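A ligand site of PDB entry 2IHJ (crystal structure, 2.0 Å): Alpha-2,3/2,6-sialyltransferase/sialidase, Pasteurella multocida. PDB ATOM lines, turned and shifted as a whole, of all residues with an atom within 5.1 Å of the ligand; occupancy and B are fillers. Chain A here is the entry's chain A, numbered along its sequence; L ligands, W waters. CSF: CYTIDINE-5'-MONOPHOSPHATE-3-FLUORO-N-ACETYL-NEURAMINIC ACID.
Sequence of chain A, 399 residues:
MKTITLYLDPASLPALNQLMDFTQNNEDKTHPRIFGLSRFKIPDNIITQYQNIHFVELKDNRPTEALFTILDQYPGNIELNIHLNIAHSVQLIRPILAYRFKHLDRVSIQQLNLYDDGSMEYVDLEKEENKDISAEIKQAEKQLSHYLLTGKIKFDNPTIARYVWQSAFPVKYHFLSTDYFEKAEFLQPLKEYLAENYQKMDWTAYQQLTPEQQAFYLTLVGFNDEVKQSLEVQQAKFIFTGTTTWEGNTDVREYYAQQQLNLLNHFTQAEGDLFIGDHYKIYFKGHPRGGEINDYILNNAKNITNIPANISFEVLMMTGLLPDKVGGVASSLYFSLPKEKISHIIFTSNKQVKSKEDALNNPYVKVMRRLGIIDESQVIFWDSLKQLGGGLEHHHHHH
Residues that only touch the ligand: Ser 12, Leu 13, Gly 118, Thr 244, Gly 286, Pro 288, Ile 311, Ser 331 and Leu 333. Hydrophobic or aromatic side chains that line the ligand: Leu 13, Met 120, Trp 246, His 287, Pro 288, Phe 313 and Leu 333. 21 residues have an atom within 4 Å of the ligand: Ser 12, Leu 13, Arg 39, Asp 117, Gly 118, Ser 119, Met 120, Gly 242, Thr 244, Trp 246, Lys 285, Gly 286, His 287, Pro 288, Ile 311, Ser 312, Phe 313, Glu 314, Ser 331, Ser 332 and Leu 333. The nearest printed residue that does not touch the ligand is Thr 243 (4.1 Å).
Water W3 lies within hydrogen-bond range of an oxygen (OBA) of the ligand (2.5 Å), the backbone carbonyl oxygen of Asp 117 (2.7 Å), the backbone NH of Ser 12 (3.2 Å) and the backbone NH of Leu 13 (3.2 Å). Water W1 lies within hydrogen-bond range of OH of Tyr 364, O2A of the ligand and OG of Ser 119. Water W7 lies within hydrogen-bond range of O8A of the ligand (2.9 Å), O of Ala 330 (2.9 Å) and OG1 of Thr 243 (2.9 Å). Water W6 bridges the side-chain hydroxyl (OG1) of Thr 243 and an oxygen (O9A) of the ligand.
N of Ser 119 sits at hydrogen-bond distance from OG of Ser 332, 2.9 Å away. OG of Ser 119 is in hydrogen-bond range of OH of Tyr 364, at 3.4 Å. NH1 of Arg 39 sits at hydrogen-bond distance from OG of Ser 12, at 2.6 Å. NZ of Lys 285 sits at hydrogen-bond distance from O of Ile 311 (2.9 Å). The side-chain amino group (NZ) of Lys 285 is in hydrogen-bond range of the backbone carbonyl oxygen (O) of Ala 309, 3.0 Å away. The side-chain hydroxyl (OG) of Ser 331 sits close to the backbone NH (N) of Leu 333, at 3.3 Å. The backbone NH (N) of Ser 331 lies close to the side-chain hydroxyl (OH) of Tyr 364 (3.4 Å). The backbone NH of Gly 118 lies within hydrogen-bond range of the side-chain carboxylate of Glu 121 (3.0 Å).
The indole nitrogen of Trp 246 is in hydrogen-bond range of an oxygen (O7A) of the ligand, 2.5 Å away. The side-chain carboxylate of Glu 314 sits at hydrogen-bond distance from an oxygen (O2') of the ligand (2.6 Å). O4A of the ligand lies within hydrogen-bond range of OD2 of Asp 117. NE2 of His 287 sits at hydrogen-bond distance from O3A of the ligand, at 2.6 Å. N of Ser 332 lies within hydrogen-bond range of O2A of the ligand, at 2.9 Å. An oxygen (O2A) of the ligand is in hydrogen-bond range of the side-chain hydroxyl (OG) of Ser 332 (3.0 Å). The backbone NH (N) of Phe 313 lies within hydrogen-bond range of an oxygen (O2) of the ligand, 2.9 Å away. The side-chain hydroxyl (OG) of Ser 119 sits at hydrogen-bond distance from a nitrogen (N5A) of the ligand (3.0 Å). NH2 of Arg 39 lies within salt-bridge range of OAA of the ligand, at 3.0 Å. N of Met 120 is in hydrogen-bond range of O4A of the ligand (3.0 Å). The backbone carbonyl oxygen (O) of Lys 285 lies within hydrogen-bond range of a nitrogen (N4) of the ligand, 3.0 Å away. An oxygen (O2) of the ligand is in hydrogen-bond range of the side-chain amino group (NZ) of Lys 285 (3.1 Å). The backbone carbonyl oxygen (O) of Gly 242 sits at hydrogen-bond distance from a nitrogen (N4) of the ligand (3.0 Å). The side-chain hydroxyl (OG) of Ser 312 sits at hydrogen-bond distance from an oxygen (O2') of the ligand, 3.1 Å away.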
ATOM      1  N   ALA A  11     -14.048 -13.944   1.140  1.00  0.00           N
ATOM      2  CA  ALA A  11     -15.436 -14.441   1.140  1.00  0.00           C
ATOM      3  C   ALA A  11     -16.490 -13.360   0.803  1.00  0.00           C
ATOM      4  O   ALA A  11     -16.232 -12.483  -0.026  1.00  0.00           O
ATOM      5  CB  ALA A  11     -15.737 -15.150   2.457  1.00  0.00           C
ATOM      6  N   SER A  12     -17.654 -13.421   1.450  1.00  0.00           N
ATOM      7  CA  SER A  12     -18.771 -12.509   1.130  1.00  0.00           C
ATOM      8  C   SER A  12     -19.130 -11.531   2.251  1.00  0.00           C
ATOM      9  O   SER A  12     -19.225 -10.319   2.022  1.00  0.00           O
ATOM     10  CB  SER A  12     -20.032 -13.286   0.745  1.00  0.00           C
ATOM     11  OG  SER A  12     -19.916 -13.872  -0.529  1.00  0.00           O
ATOM     12  N   LEU A  13     -19.360 -12.075   3.443  1.00  0.00           N
ATOM     13  CA  LEU A  13     -19.931 -11.303   4.550  1.00  0.00           C
ATOM     14  C   LEU A  13     -19.033 -10.170   5.109  1.00  0.00           C
ATOM     15  O   LEU A  13     -19.516  -9.054   5.303  1.00  0.00           O
ATOM     16  CB  LEU A  13     -20.438 -12.254   5.653  1.00  0.00           C
ATOM     17  CG  LEU A  13     -21.693 -11.953   6.461  1.00  0.00           C
ATOM     18  CD1 LEU A  13     -22.944 -11.717   5.596  1.00  0.00           C
ATOM     19  CD2 LEU A  13     -21.947 -13.104   7.447  1.00  0.00           C
ATOM     20  N   LEU A  16     -19.011  -7.311   2.530  1.00  0.00           N
ATOM     21  CA  LEU A  16     -20.270  -6.568   2.530  1.00  0.00           C
ATOM     22  C   LEU A  16     -20.249  -5.455   3.593  1.00  0.00           C
ATOM     23  O   LEU A  16     -20.639  -4.311   3.316  1.00  0.00           O
ATOM     24  CB  LEU A  16     -21.447  -7.531   2.750  1.00  0.00           C
ATOM     25  CG  LEU A  16     -22.863  -7.232   2.257  1.00  0.00           C
ATOM     26  CD1 LEU A  16     -22.908  -7.101   0.746  1.00  0.00           C
ATOM     27  CD2 LEU A  16     -23.810  -8.358   2.718  1.00  0.00           C
ATOM     28  N   ARG A  39     -14.425 -11.406  -4.033  1.00  0.00           N
ATOM     29  CA  ARG A  39     -15.769 -11.582  -4.584  1.00  0.00           C
ATOM     30  C   ARG A  39     -16.414 -10.295  -5.111  1.00  0.00           C
ATOM     31  O   ARG A  39     -17.528 -10.340  -5.645  1.00  0.00           O
ATOM     32  CB  ARG A  39     -16.684 -12.294  -3.569  1.00  0.00           C
ATOM     33  CG  ARG A  39     -16.268 -13.745  -3.264  1.00  0.00           C
ATOM     34  CD  ARG A  39     -17.416 -14.587  -2.666  1.00  0.00           C
ATOM     35  NE  ARG A  39     -16.933 -15.869  -2.156  1.00  0.00           N
ATOM     36  CZ  ARG A  39     -17.555 -16.602  -1.230  1.00  0.00           C
ATOM     37  NH1 ARG A  39     -18.707 -16.198  -0.693  1.00  0.00           N
ATOM     38  NH2 ARG A  39     -17.024 -17.755  -0.821  1.00  0.00           N
ATOM     39  N   ASP A 117     -16.531 -14.381   8.829  1.00  0.00           N
ATOM     40  CA  ASP A 117     -16.679 -15.165   7.579  1.00  0.00           C
ATOM     41  C   ASP A 117     -18.128 -15.662   7.444  1.00  0.00           C
ATOM     42  O   ASP A 117     -18.712 -15.604   6.342  1.00  0.00           O
ATOM     43  CB  ASP A 117     -15.670 -16.345   7.635  1.00  0.00           C
ATOM     44  CG  ASP A 117     -15.588 -17.162   6.332  1.00  0.00           C
ATOM     45  OD1 ASP A 117     -14.837 -16.791   5.401  1.00  0.00           O
ATOM     46  OD2 ASP A 117     -16.222 -18.235   6.278  1.00  0.00           O
ATOM     47  N   GLY A 118     -18.713 -16.114   8.552  1.00  0.00           N
ATOM     48  CA  GLY A 118     -20.118 -16.568   8.588  1.00  0.00           C
ATOM     49  C   GLY A 118     -20.360 -17.692   9.585  1.00  0.00           C
ATOM     50  O   GLY A 118     -19.909 -17.614  10.734  1.00  0.00           O
ATOM     51  N   SER A 119     -21.066 -18.732   9.144  1.00  0.00           N
ATOM     52  CA  SER A 119     -21.363 -19.903   9.977  1.00  0.00           C
ATOM     53  C   SER A 119     -20.123 -20.675  10.424  1.00  0.00           C
ATOM     54  O   SER A 119     -20.154 -21.336  11.456  1.00  0.00           O
ATOM     55  CB  SER A 119     -22.347 -20.869   9.282  1.00  0.00           C
ATOM     56  OG  SER A 119     -21.790 -21.422   8.097  1.00  0.00           O
ATOM     57  N   MET A 120     -19.049 -20.579   9.635  1.00  0.00           N
ATOM     58  CA  MET A 120     -17.767 -21.239   9.957  1.00  0.00           C
ATOM     59  C   MET A 120     -17.271 -20.997  11.375  1.00  0.00           C
ATOM     60  O   MET A 120     -16.943 -21.964  12.084  1.00  0.00           O
ATOM     61  CB  MET A 120     -16.677 -20.860   8.933  1.00  0.00           C
ATOM     62  CG  MET A 120     -15.327 -21.556   9.176  1.00  0.00           C
ATOM     63  SD  MET A 120     -14.133 -21.244   7.853  1.00  0.00           S
ATOM     64  CE  MET A 120     -14.745 -22.397   6.646  1.00  0.00           C
ATOM     65  N   GLU A 121     -17.202 -19.726  11.797  1.00  0.00           N
ATOM     66  CA  GLU A 121     -16.714 -19.369  13.141  1.00  0.00           C
ATOM     67  C   GLU A 121     -17.517 -20.052  14.266  1.00  0.00           C
ATOM     68  O   GLU A 121     -16.949 -20.469  15.282  1.00  0.00           O
ATOM     69  CB  GLU A 121     -16.680 -17.846  13.368  1.00  0.00           C
ATOM     70  CG  GLU A 121     -15.511 -17.094  12.691  1.00  0.00           C
ATOM     71  CD  GLU A 121     -15.839 -16.592  11.290  1.00  0.00           C
ATOM     72  OE1 GLU A 121     -16.853 -17.047  10.708  1.00  0.00           O
ATOM     73  OE2 GLU A 121     -15.088 -15.738  10.760  1.00  0.00           O
ATOM     74  N   VAL A 123     -19.656 -22.947  13.955  1.00  0.00           N
ATOM     75  CA  VAL A 123     -19.416 -24.400  13.863  1.00  0.00           C
ATOM     76  C   VAL A 123     -18.060 -24.753  14.513  1.00  0.00           C
ATOM     77  O   VAL A 123     -17.962 -25.734  15.253  1.00  0.00           O
ATOM     78  CB  VAL A 123     -19.524 -24.920  12.390  1.00  0.00           C
ATOM     79  CG1 VAL A 123     -18.859 -26.294  12.229  1.00  0.00           C
ATOM     80  CG2 VAL A 123     -20.983 -24.979  11.933  1.00  0.00           C
ATOM     81  N   THR A 241     -33.096 -21.111  -1.782  1.00  0.00           N
ATOM     82  CA  THR A 241     -31.698 -20.732  -1.615  1.00  0.00           C
ATOM     83  C   THR A 241     -30.753 -21.923  -1.846  1.00  0.00           C
ATOM     84  O   THR A 241     -30.958 -23.000  -1.265  1.00  0.00           O
ATOM     85  CB  THR A 241     -31.407 -20.121  -0.211  1.00  0.00           C
ATOM     86  OG1 THR A 241     -31.534 -21.131   0.802  1.00  0.00           O
ATOM     87  CG2 THR A 241     -32.357 -18.973   0.085  1.00  0.00           C
ATOM     88  N   GLY A 242     -29.744 -21.724  -2.682  1.00  0.00           N
ATOM     89  CA  GLY A 242     -28.802 -22.785  -3.027  1.00  0.00           C
ATOM     90  C   GLY A 242     -27.537 -22.832  -2.182  1.00  0.00           C
ATOM     91  O   GLY A 242     -27.261 -21.920  -1.401  1.00  0.00           O
ATOM     92  N   THR A 243     -26.776 -23.913  -2.354  1.00  0.00           N
ATOM     93  CA  THR A 243     -25.518 -24.119  -1.649  1.00  0.00           C
ATOM     94  C   THR A 243     -24.393 -24.421  -2.656  1.00  0.00           C
ATOM     95  O   THR A 243     -24.616 -24.366  -3.882  1.00  0.00           O
ATOM     96  CB  THR A 243     -25.648 -25.248  -0.570  1.00  0.00           C
ATOM     97  OG1 THR A 243     -24.481 -25.284   0.265  1.00  0.00           O
ATOM     98  CG2 THR A 243     -25.882 -26.628  -1.213  1.00  0.00           C
ATOM     99  N   THR A 244     -23.202 -24.724  -2.144  1.00  0.00           N
ATOM    100  CA  THR A 244     -22.096 -25.176  -2.967  1.00  0.00           C
ATOM    101  C   THR A 244     -21.258 -26.213  -2.224  1.00  0.00           C
ATOM    102  O   THR A 244     -21.479 -26.478  -1.037  1.00  0.00           O
ATOM    103  CB  THR A 244     -21.203 -23.995  -3.461  1.00  0.00           C
ATOM    104  OG1 THR A 244     -20.344 -24.448  -4.514  1.00  0.00           O
ATOM    105  CG2 THR A 244     -20.339 -23.430  -2.320  1.00  0.00           C
ATOM    106  N   TRP A 246     -16.929 -27.105  -1.822  1.00  0.00           N
ATOM    107  CA  TRP A 246     -15.576 -26.659  -2.138  1.00  0.00           C
ATOM    108  C   TRP A 246     -14.729 -27.829  -2.628  1.00  0.00           C
ATOM    109  O   TRP A 246     -13.534 -27.685  -2.897  1.00  0.00           O
ATOM    110  CB  TRP A 246     -14.915 -25.947  -0.940  1.00  0.00           C
ATOM    111  CG  TRP A 246     -15.821 -24.931  -0.295  1.00  0.00           C
ATOM    112  CD1 TRP A 246     -16.366 -25.000   0.946  1.00  0.00           C
ATOM    113  CD2 TRP A 246     -16.299 -23.705  -0.872  1.00  0.00           C
ATOM    114  NE1 TRP A 246     -17.143 -23.892   1.188  1.00  0.00           N
ATOM    115  CE2 TRP A 246     -17.120 -23.080   0.095  1.00  0.00           C
ATOM    116  CE3 TRP A 246     -16.105 -23.067  -2.112  1.00  0.00           C
ATOM    117  CZ2 TRP A 246     -17.752 -21.857  -0.142  1.00  0.00           C
ATOM    118  CZ3 TRP A 246     -16.737 -21.845  -2.335  1.00  0.00           C
ATOM    119  CH2 TRP A 246     -17.546 -21.255  -1.360  1.00  0.00           C
ATOM    120  N   LYS A 285     -32.201 -18.190  -5.632  1.00  0.00           N
ATOM    121  CA  LYS A 285     -31.049 -17.404  -5.199  1.00  0.00           C
ATOM    122  C   LYS A 285     -29.893 -18.380  -4.969  1.00  0.00           C
ATOM    123  O   LYS A 285     -29.739 -18.934  -3.881  1.00  0.00           O
ATOM    124  CB  LYS A 285     -31.374 -16.585  -3.919  1.00  0.00           C
ATOM    125  CG  LYS A 285     -30.217 -15.787  -3.255  1.00  0.00           C
ATOM    126  CD  LYS A 285     -29.741 -14.560  -4.068  1.00  0.00           C
ATOM    127  CE  LYS A 285     -28.450 -14.844  -4.832  1.00  0.00           C
ATOM    128  NZ  LYS A 285     -27.257 -14.947  -3.915  1.00  0.00           N
ATOM    129  N   GLY A 286     -29.094 -18.595  -6.012  1.00  0.00           N
ATOM    130  CA  GLY A 286     -27.947 -19.506  -5.928  1.00  0.00           C
ATOM    131  C   GLY A 286     -26.801 -18.976  -5.072  1.00  0.00           C
ATOM    132  O   GLY A 286     -26.678 -17.765  -4.834  1.00  0.00           O
ATOM    133  N   HIS A 287     -25.953 -19.892  -4.610  1.00  0.00           N
ATOM    134  CA  HIS A 287     -24.733 -19.533  -3.869  1.00  0.00           C
ATOM    135  C   HIS A 287     -23.782 -18.749  -4.795  1.00  0.00           C
ATOM    136  O   HIS A 287     -23.637 -19.098  -5.966  1.00  0.00           O
ATOM    137  CB  HIS A 287     -24.053 -20.798  -3.325  1.00  0.00           C
ATOM    138  CG  HIS A 287     -22.978 -20.521  -2.336  1.00  0.00           C
ATOM    139  ND1 HIS A 287     -21.712 -20.118  -2.700  1.00  0.00           N
ATOM    140  CD2 HIS A 287     -22.971 -20.566  -0.975  1.00  0.00           C
ATOM    141  CE1 HIS A 287     -20.980 -19.932  -1.618  1.00  0.00           C
ATOM    142  NE2 HIS A 287     -21.724 -20.192  -0.555  1.00  0.00           N
ATOM    143  N   PRO A 288     -23.109 -17.686  -4.270  1.00  0.00           N
ATOM    144  CA  PRO A 288     -22.186 -16.897  -5.101  1.00  0.00           C
ATOM    145  C   PRO A 288     -21.098 -17.721  -5.826  1.00  0.00           C
ATOM    146  O   PRO A 288     -20.621 -17.287  -6.877  1.00  0.00           O
ATOM    147  CB  PRO A 288     -21.531 -15.928  -4.104  1.00  0.00           C
ATOM    148  CG  PRO A 288     -22.489 -15.835  -2.978  1.00  0.00           C
ATOM    149  CD  PRO A 288     -23.194 -17.162  -2.900  1.00  0.00           C
ATOM    150  N   ALA A 309     -26.622 -14.645  -8.682  1.00  0.00           N
ATOM    151  CA  ALA A 309     -25.980 -15.316  -7.545  1.00  0.00           C
ATOM    152  C   ALA A 309     -24.994 -14.439  -6.764  1.00  0.00           C
ATOM    153  O   ALA A 309     -24.805 -14.653  -5.556  1.00  0.00           O
ATOM    154  CB  ALA A 309     -25.310 -16.623  -8.010  1.00  0.00           C
ATOM    155  N   ILE A 311     -25.355 -11.384  -5.826  1.00  0.00           N
ATOM    156  CA  ILE A 311     -26.042 -10.437  -4.932  1.00  0.00           C
ATOM    157  C   ILE A 311     -26.285 -11.096  -3.565  1.00  0.00           C
ATOM    158  O   ILE A 311     -27.027 -12.075  -3.487  1.00  0.00           O
ATOM    159  CB  ILE A 311     -27.393  -9.954  -5.561  1.00  0.00           C
ATOM    160  CG1 ILE A 311     -27.126  -9.265  -6.909  1.00  0.00           C
ATOM    161  CG2 ILE A 311     -28.153  -9.027  -4.597  1.00  0.00           C
ATOM    162  CD1 ILE A 311     -28.359  -9.016  -7.779  1.00  0.00           C
ATOM    163  N   SER A 312     -25.660 -10.570  -2.518  1.00  0.00           N
ATOM    164  CA  SER A 312     -25.835 -11.116  -1.156  1.00  0.00           C
ATOM    165  C   SER A 312     -27.281 -11.000  -0.689  1.00  0.00           C
ATOM    166  O   SER A 312     -27.898  -9.939  -0.817  1.00  0.00           O
ATOM    167  CB  SER A 312     -24.912 -10.412  -0.152  1.00  0.00           C
ATOM    168  OG  SER A 312     -23.604 -10.953  -0.176  1.00  0.00           O
ATOM    169  N   PHE A 313     -27.810 -12.099  -0.154  1.00  0.00           N
ATOM    170  CA  PHE A 313     -29.191 -12.157   0.347  1.00  0.00           C
ATOM    171  C   PHE A 313     -29.555 -10.987   1.278  1.00  0.00           C
ATOM    172  O   PHE A 313     -30.648 -10.403   1.147  1.00  0.00           O
ATOM    173  CB  PHE A 313     -29.449 -13.509   1.042  1.00  0.00           C
ATOM    174  CG  PHE A 313     -30.894 -13.718   1.449  1.00  0.00           C
ATOM    175  CD1 PHE A 313     -31.362 -13.246   2.676  1.00  0.00           C
ATOM    176  CD2 PHE A 313     -31.779 -14.372   0.595  1.00  0.00           C
ATOM    177  CE1 PHE A 313     -32.699 -13.428   3.049  1.00  0.00           C
ATOM    178  CE2 PHE A 313     -33.116 -14.565   0.959  1.00  0.00           C
ATOM    179  CZ  PHE A 313     -33.578 -14.085   2.187  1.00  0.00           C
ATOM    180  N   GLU A 314     -28.644 -10.631   2.183  1.00  0.00           N
ATOM    181  CA  GLU A 314     -28.855  -9.568   3.186  1.00  0.00           C
ATOM    182  C   GLU A 314     -29.207  -8.196   2.608  1.00  0.00           C
ATOM    183  O   GLU A 314     -29.834  -7.385   3.300  1.00  0.00           O
ATOM    184  CB  GLU A 314     -27.641  -9.430   4.120  1.00  0.00           C
ATOM    185  CG  GLU A 314     -27.347 -10.657   5.002  1.00  0.00           C
ATOM    186  CD  GLU A 314     -26.610 -11.776   4.272  1.00  0.00           C
ATOM    187  OE1 GLU A 314     -26.479 -12.879   4.848  1.00  0.00           O
ATOM    188  OE2 GLU A 314     -26.150 -11.574   3.126  1.00  0.00           O
ATOM    189  N   ALA A 330     -29.037 -25.302   4.608  1.00  0.00           N
ATOM    190  CA  ALA A 330     -28.454 -24.478   5.682  1.00  0.00           C
ATOM    191  C   ALA A 330     -27.369 -23.505   5.172  1.00  0.00           C
ATOM    192  O   ALA A 330     -26.422 -23.928   4.494  1.00  0.00           O
ATOM    193  CB  ALA A 330     -27.892 -25.376   6.806  1.00  0.00           C
ATOM    194  N   SER A 331     -27.551 -22.212   5.481  1.00  0.00           N
ATOM    195  CA  SER A 331     -26.651 -21.140   5.020  1.00  0.00           C
ATOM    196  C   SER A 331     -26.515 -20.024   6.088  1.00  0.00           C
ATOM    197  O   SER A 331     -27.357 -19.917   6.984  1.00  0.00           O
ATOM    198  CB  SER A 331     -27.169 -20.542   3.703  1.00  0.00           C
ATOM    199  OG  SER A 331     -26.480 -19.348   3.353  1.00  0.00           O
ATOM    200  N   SER A 332     -25.461 -19.209   5.961  1.00  0.00           N
ATOM    201  CA  SER A 332     -25.232 -18.057   6.840  1.00  0.00           C
ATOM    202  C   SER A 332     -26.362 -17.009   6.757  1.00  0.00           C
ATOM    203  O   SER A 332     -26.567 -16.223   7.686  1.00  0.00           O
ATOM    204  CB  SER A 332     -23.887 -17.370   6.520  1.00  0.00           C
ATOM    205  OG  SER A 332     -22.777 -18.212   6.809  1.00  0.00           O
ATOM    206  N   LEU A 333     -27.085 -16.998   5.635  1.00  0.00           N
ATOM    207  CA  LEU A 333     -28.176 -16.058   5.427  1.00  0.00           C
ATOM    208  C   LEU A 333     -29.313 -16.231   6.456  1.00  0.00           C
ATOM    209  O   LEU A 333     -29.971 -15.253   6.832  1.00  0.00           O
ATOM    210  CB  LEU A 333     -28.686 -16.124   3.973  1.00  0.00           C
ATOM    211  CG  LEU A 333     -29.490 -17.334   3.485  1.00  0.00           C
ATOM    212  CD1 LEU A 333     -30.992 -17.191   3.786  1.00  0.00           C
ATOM    213  CD2 LEU A 333     -29.290 -17.524   1.973  1.00  0.00           C
ATOM    214  N   TYR A 364     -23.269 -28.116  13.048  1.00  0.00           N
ATOM    215  CA  TYR A 364     -24.110 -27.082  12.419  1.00  0.00           C
ATOM    216  C   TYR A 364     -25.548 -27.145  12.971  1.00  0.00           C
ATOM    217  O   TYR A 364     -26.131 -26.118  13.331  1.00  0.00           O
ATOM    218  CB  TYR A 364     -24.101 -27.221  10.891  1.00  0.00           C
ATOM    219  CG  TYR A 364     -24.376 -25.932  10.090  1.00  0.00           C
ATOM    220  CD1 TYR A 364     -24.158 -25.894   8.701  1.00  0.00           C
ATOM    221  CD2 TYR A 364     -24.811 -24.753  10.709  1.00  0.00           C
ATOM    222  CE1 TYR A 364     -24.408 -24.730   7.951  1.00  0.00           C
ATOM    223  CE2 TYR A 364     -25.043 -23.578   9.967  1.00  0.00           C
ATOM    224  CZ  TYR A 364     -24.842 -23.579   8.593  1.00  0.00           C
ATOM    225  OH  TYR A 364     -25.079 -22.428   7.870  1.00  0.00           O
HETATM  226  C5A CSF L   1     -18.887 -21.309   5.355  1.00  0.00           C
HETATM  227  C4A CSF L   1     -19.087 -19.825   5.710  1.00  0.00           C
HETATM  228  C2A CSF L   1     -19.626 -19.271   3.376  1.00  0.00           C
HETATM  229  O6A CSF L   1     -19.512 -20.679   3.085  1.00  0.00           O
HETATM  230  C6A CSF L   1     -19.794 -21.599   4.145  1.00  0.00           C
HETATM  231  C3A CSF L   1     -18.668 -18.959   4.523  1.00  0.00           C
HETATM  232  O4A CSF L   1     -18.435 -19.404   6.918  1.00  0.00           O
HETATM  233  N5A CSF L   1     -19.400 -22.108   6.461  1.00  0.00           N
HETATM  234  C7A CSF L   1     -19.732 -23.026   3.567  1.00  0.00           C
HETATM  235  C8A CSF L   1     -20.635 -23.180   2.336  1.00  0.00           C
HETATM  236  C9A CSF L   1     -20.552 -24.559   1.664  1.00  0.00           C
HETATM  237  O9A CSF L   1     -21.110 -25.550   2.525  1.00  0.00           O
HETATM  238  O8A CSF L   1     -22.004 -22.927   2.681  1.00  0.00           O
HETATM  239  O7A CSF L   1     -18.374 -23.321   3.230  1.00  0.00           O
HETATM  240  C1A CSF L   1     -19.231 -18.490   2.126  1.00  0.00           C
HETATM  241  OBA CSF L   1     -19.211 -17.248   2.149  1.00  0.00           O
HETATM  242  OAA CSF L   1     -18.919 -19.113   1.085  1.00  0.00           O
HETATM  243  O1A CSF L   1     -20.941 -18.891   3.854  1.00  0.00           O
HETATM  244  O2A CSF L   1     -23.137 -19.980   4.464  1.00  0.00           O
HETATM  245  N1  CSF L   1     -25.222 -16.158   0.119  1.00  0.00           N
HETATM  246  C2  CSF L   1     -26.265 -15.747  -0.750  1.00  0.00           C
HETATM  247  N3  CSF L   1     -27.084 -16.678  -1.300  1.00  0.00           N
HETATM  248  C4  CSF L   1     -26.925 -18.001  -1.047  1.00  0.00           C
HETATM  249  C5  CSF L   1     -25.904 -18.421  -0.178  1.00  0.00           C
HETATM  250  C6  CSF L   1     -25.062 -17.471   0.381  1.00  0.00           C
HETATM  251  C3' CSF L   1     -24.386 -15.235   3.068  1.00  0.00           C
HETATM  252  C2' CSF L   1     -24.948 -14.443   1.906  1.00  0.00           C
HETATM  253  C1' CSF L   1     -24.322 -15.129   0.705  1.00  0.00           C
HETATM  254  O4' CSF L   1     -23.083 -15.694   1.179  1.00  0.00           O
HETATM  255  C4' CSF L   1     -22.968 -15.504   2.598  1.00  0.00           C
HETATM  256  PA  CSF L   1     -22.404 -19.365   3.301  1.00  0.00           P
HETATM  257  O5' CSF L   1     -23.085 -17.918   3.037  1.00  0.00           O
HETATM  258  C5' CSF L   1     -22.326 -16.724   3.266  1.00  0.00           C
HETATM  259  O3' CSF L   1     -24.423 -14.516   4.312  1.00  0.00           O
HETATM  260  O2' CSF L   1     -24.460 -13.093   1.958  1.00  0.00           O
HETATM  261  N4  CSF L   1     -27.755 -18.924  -1.595  1.00  0.00           N
HETATM  262  O2  CSF L   1     -26.413 -14.520  -0.998  1.00  0.00           O
HETATM  263  O3A CSF L   1     -22.178 -20.102   2.022  1.00  0.00           O
HETATM  264  C10 CSF L   1     -18.804 -23.219   6.940  1.00  0.00           C
HETATM  265  O10 CSF L   1     -17.759 -23.669   6.484  1.00  0.00           O
HETATM  266  C11 CSF L   1     -19.520 -23.891   8.072  1.00  0.00           C
HETATM  267  F3A CSF L   1     -17.364 -19.195   4.126  1.00  0.00           F
HETATM  268  O   HOH W   1     -23.350 -22.226   5.893  1.00  0.00           O
HETATM  269  O   HOH W   2     -22.503 -24.884   4.866  1.00  0.00           O
HETATM  270  O   HOH W   3     -19.003 -15.256   3.631  1.00  0.00           O
HETATM  271  O   HOH W   4     -15.086 -20.893   2.277  1.00  0.00           O
HETATM  272  O   HOH W   5     -21.458 -28.524   1.932  1.00  0.00           O
HETATM  273  O   HOH W   6     -23.716 -27.235   2.115  1.00  0.00           O
HETATM  274  O   HOH W   7     -24.806 -23.224   2.251  1.00  0.00           O
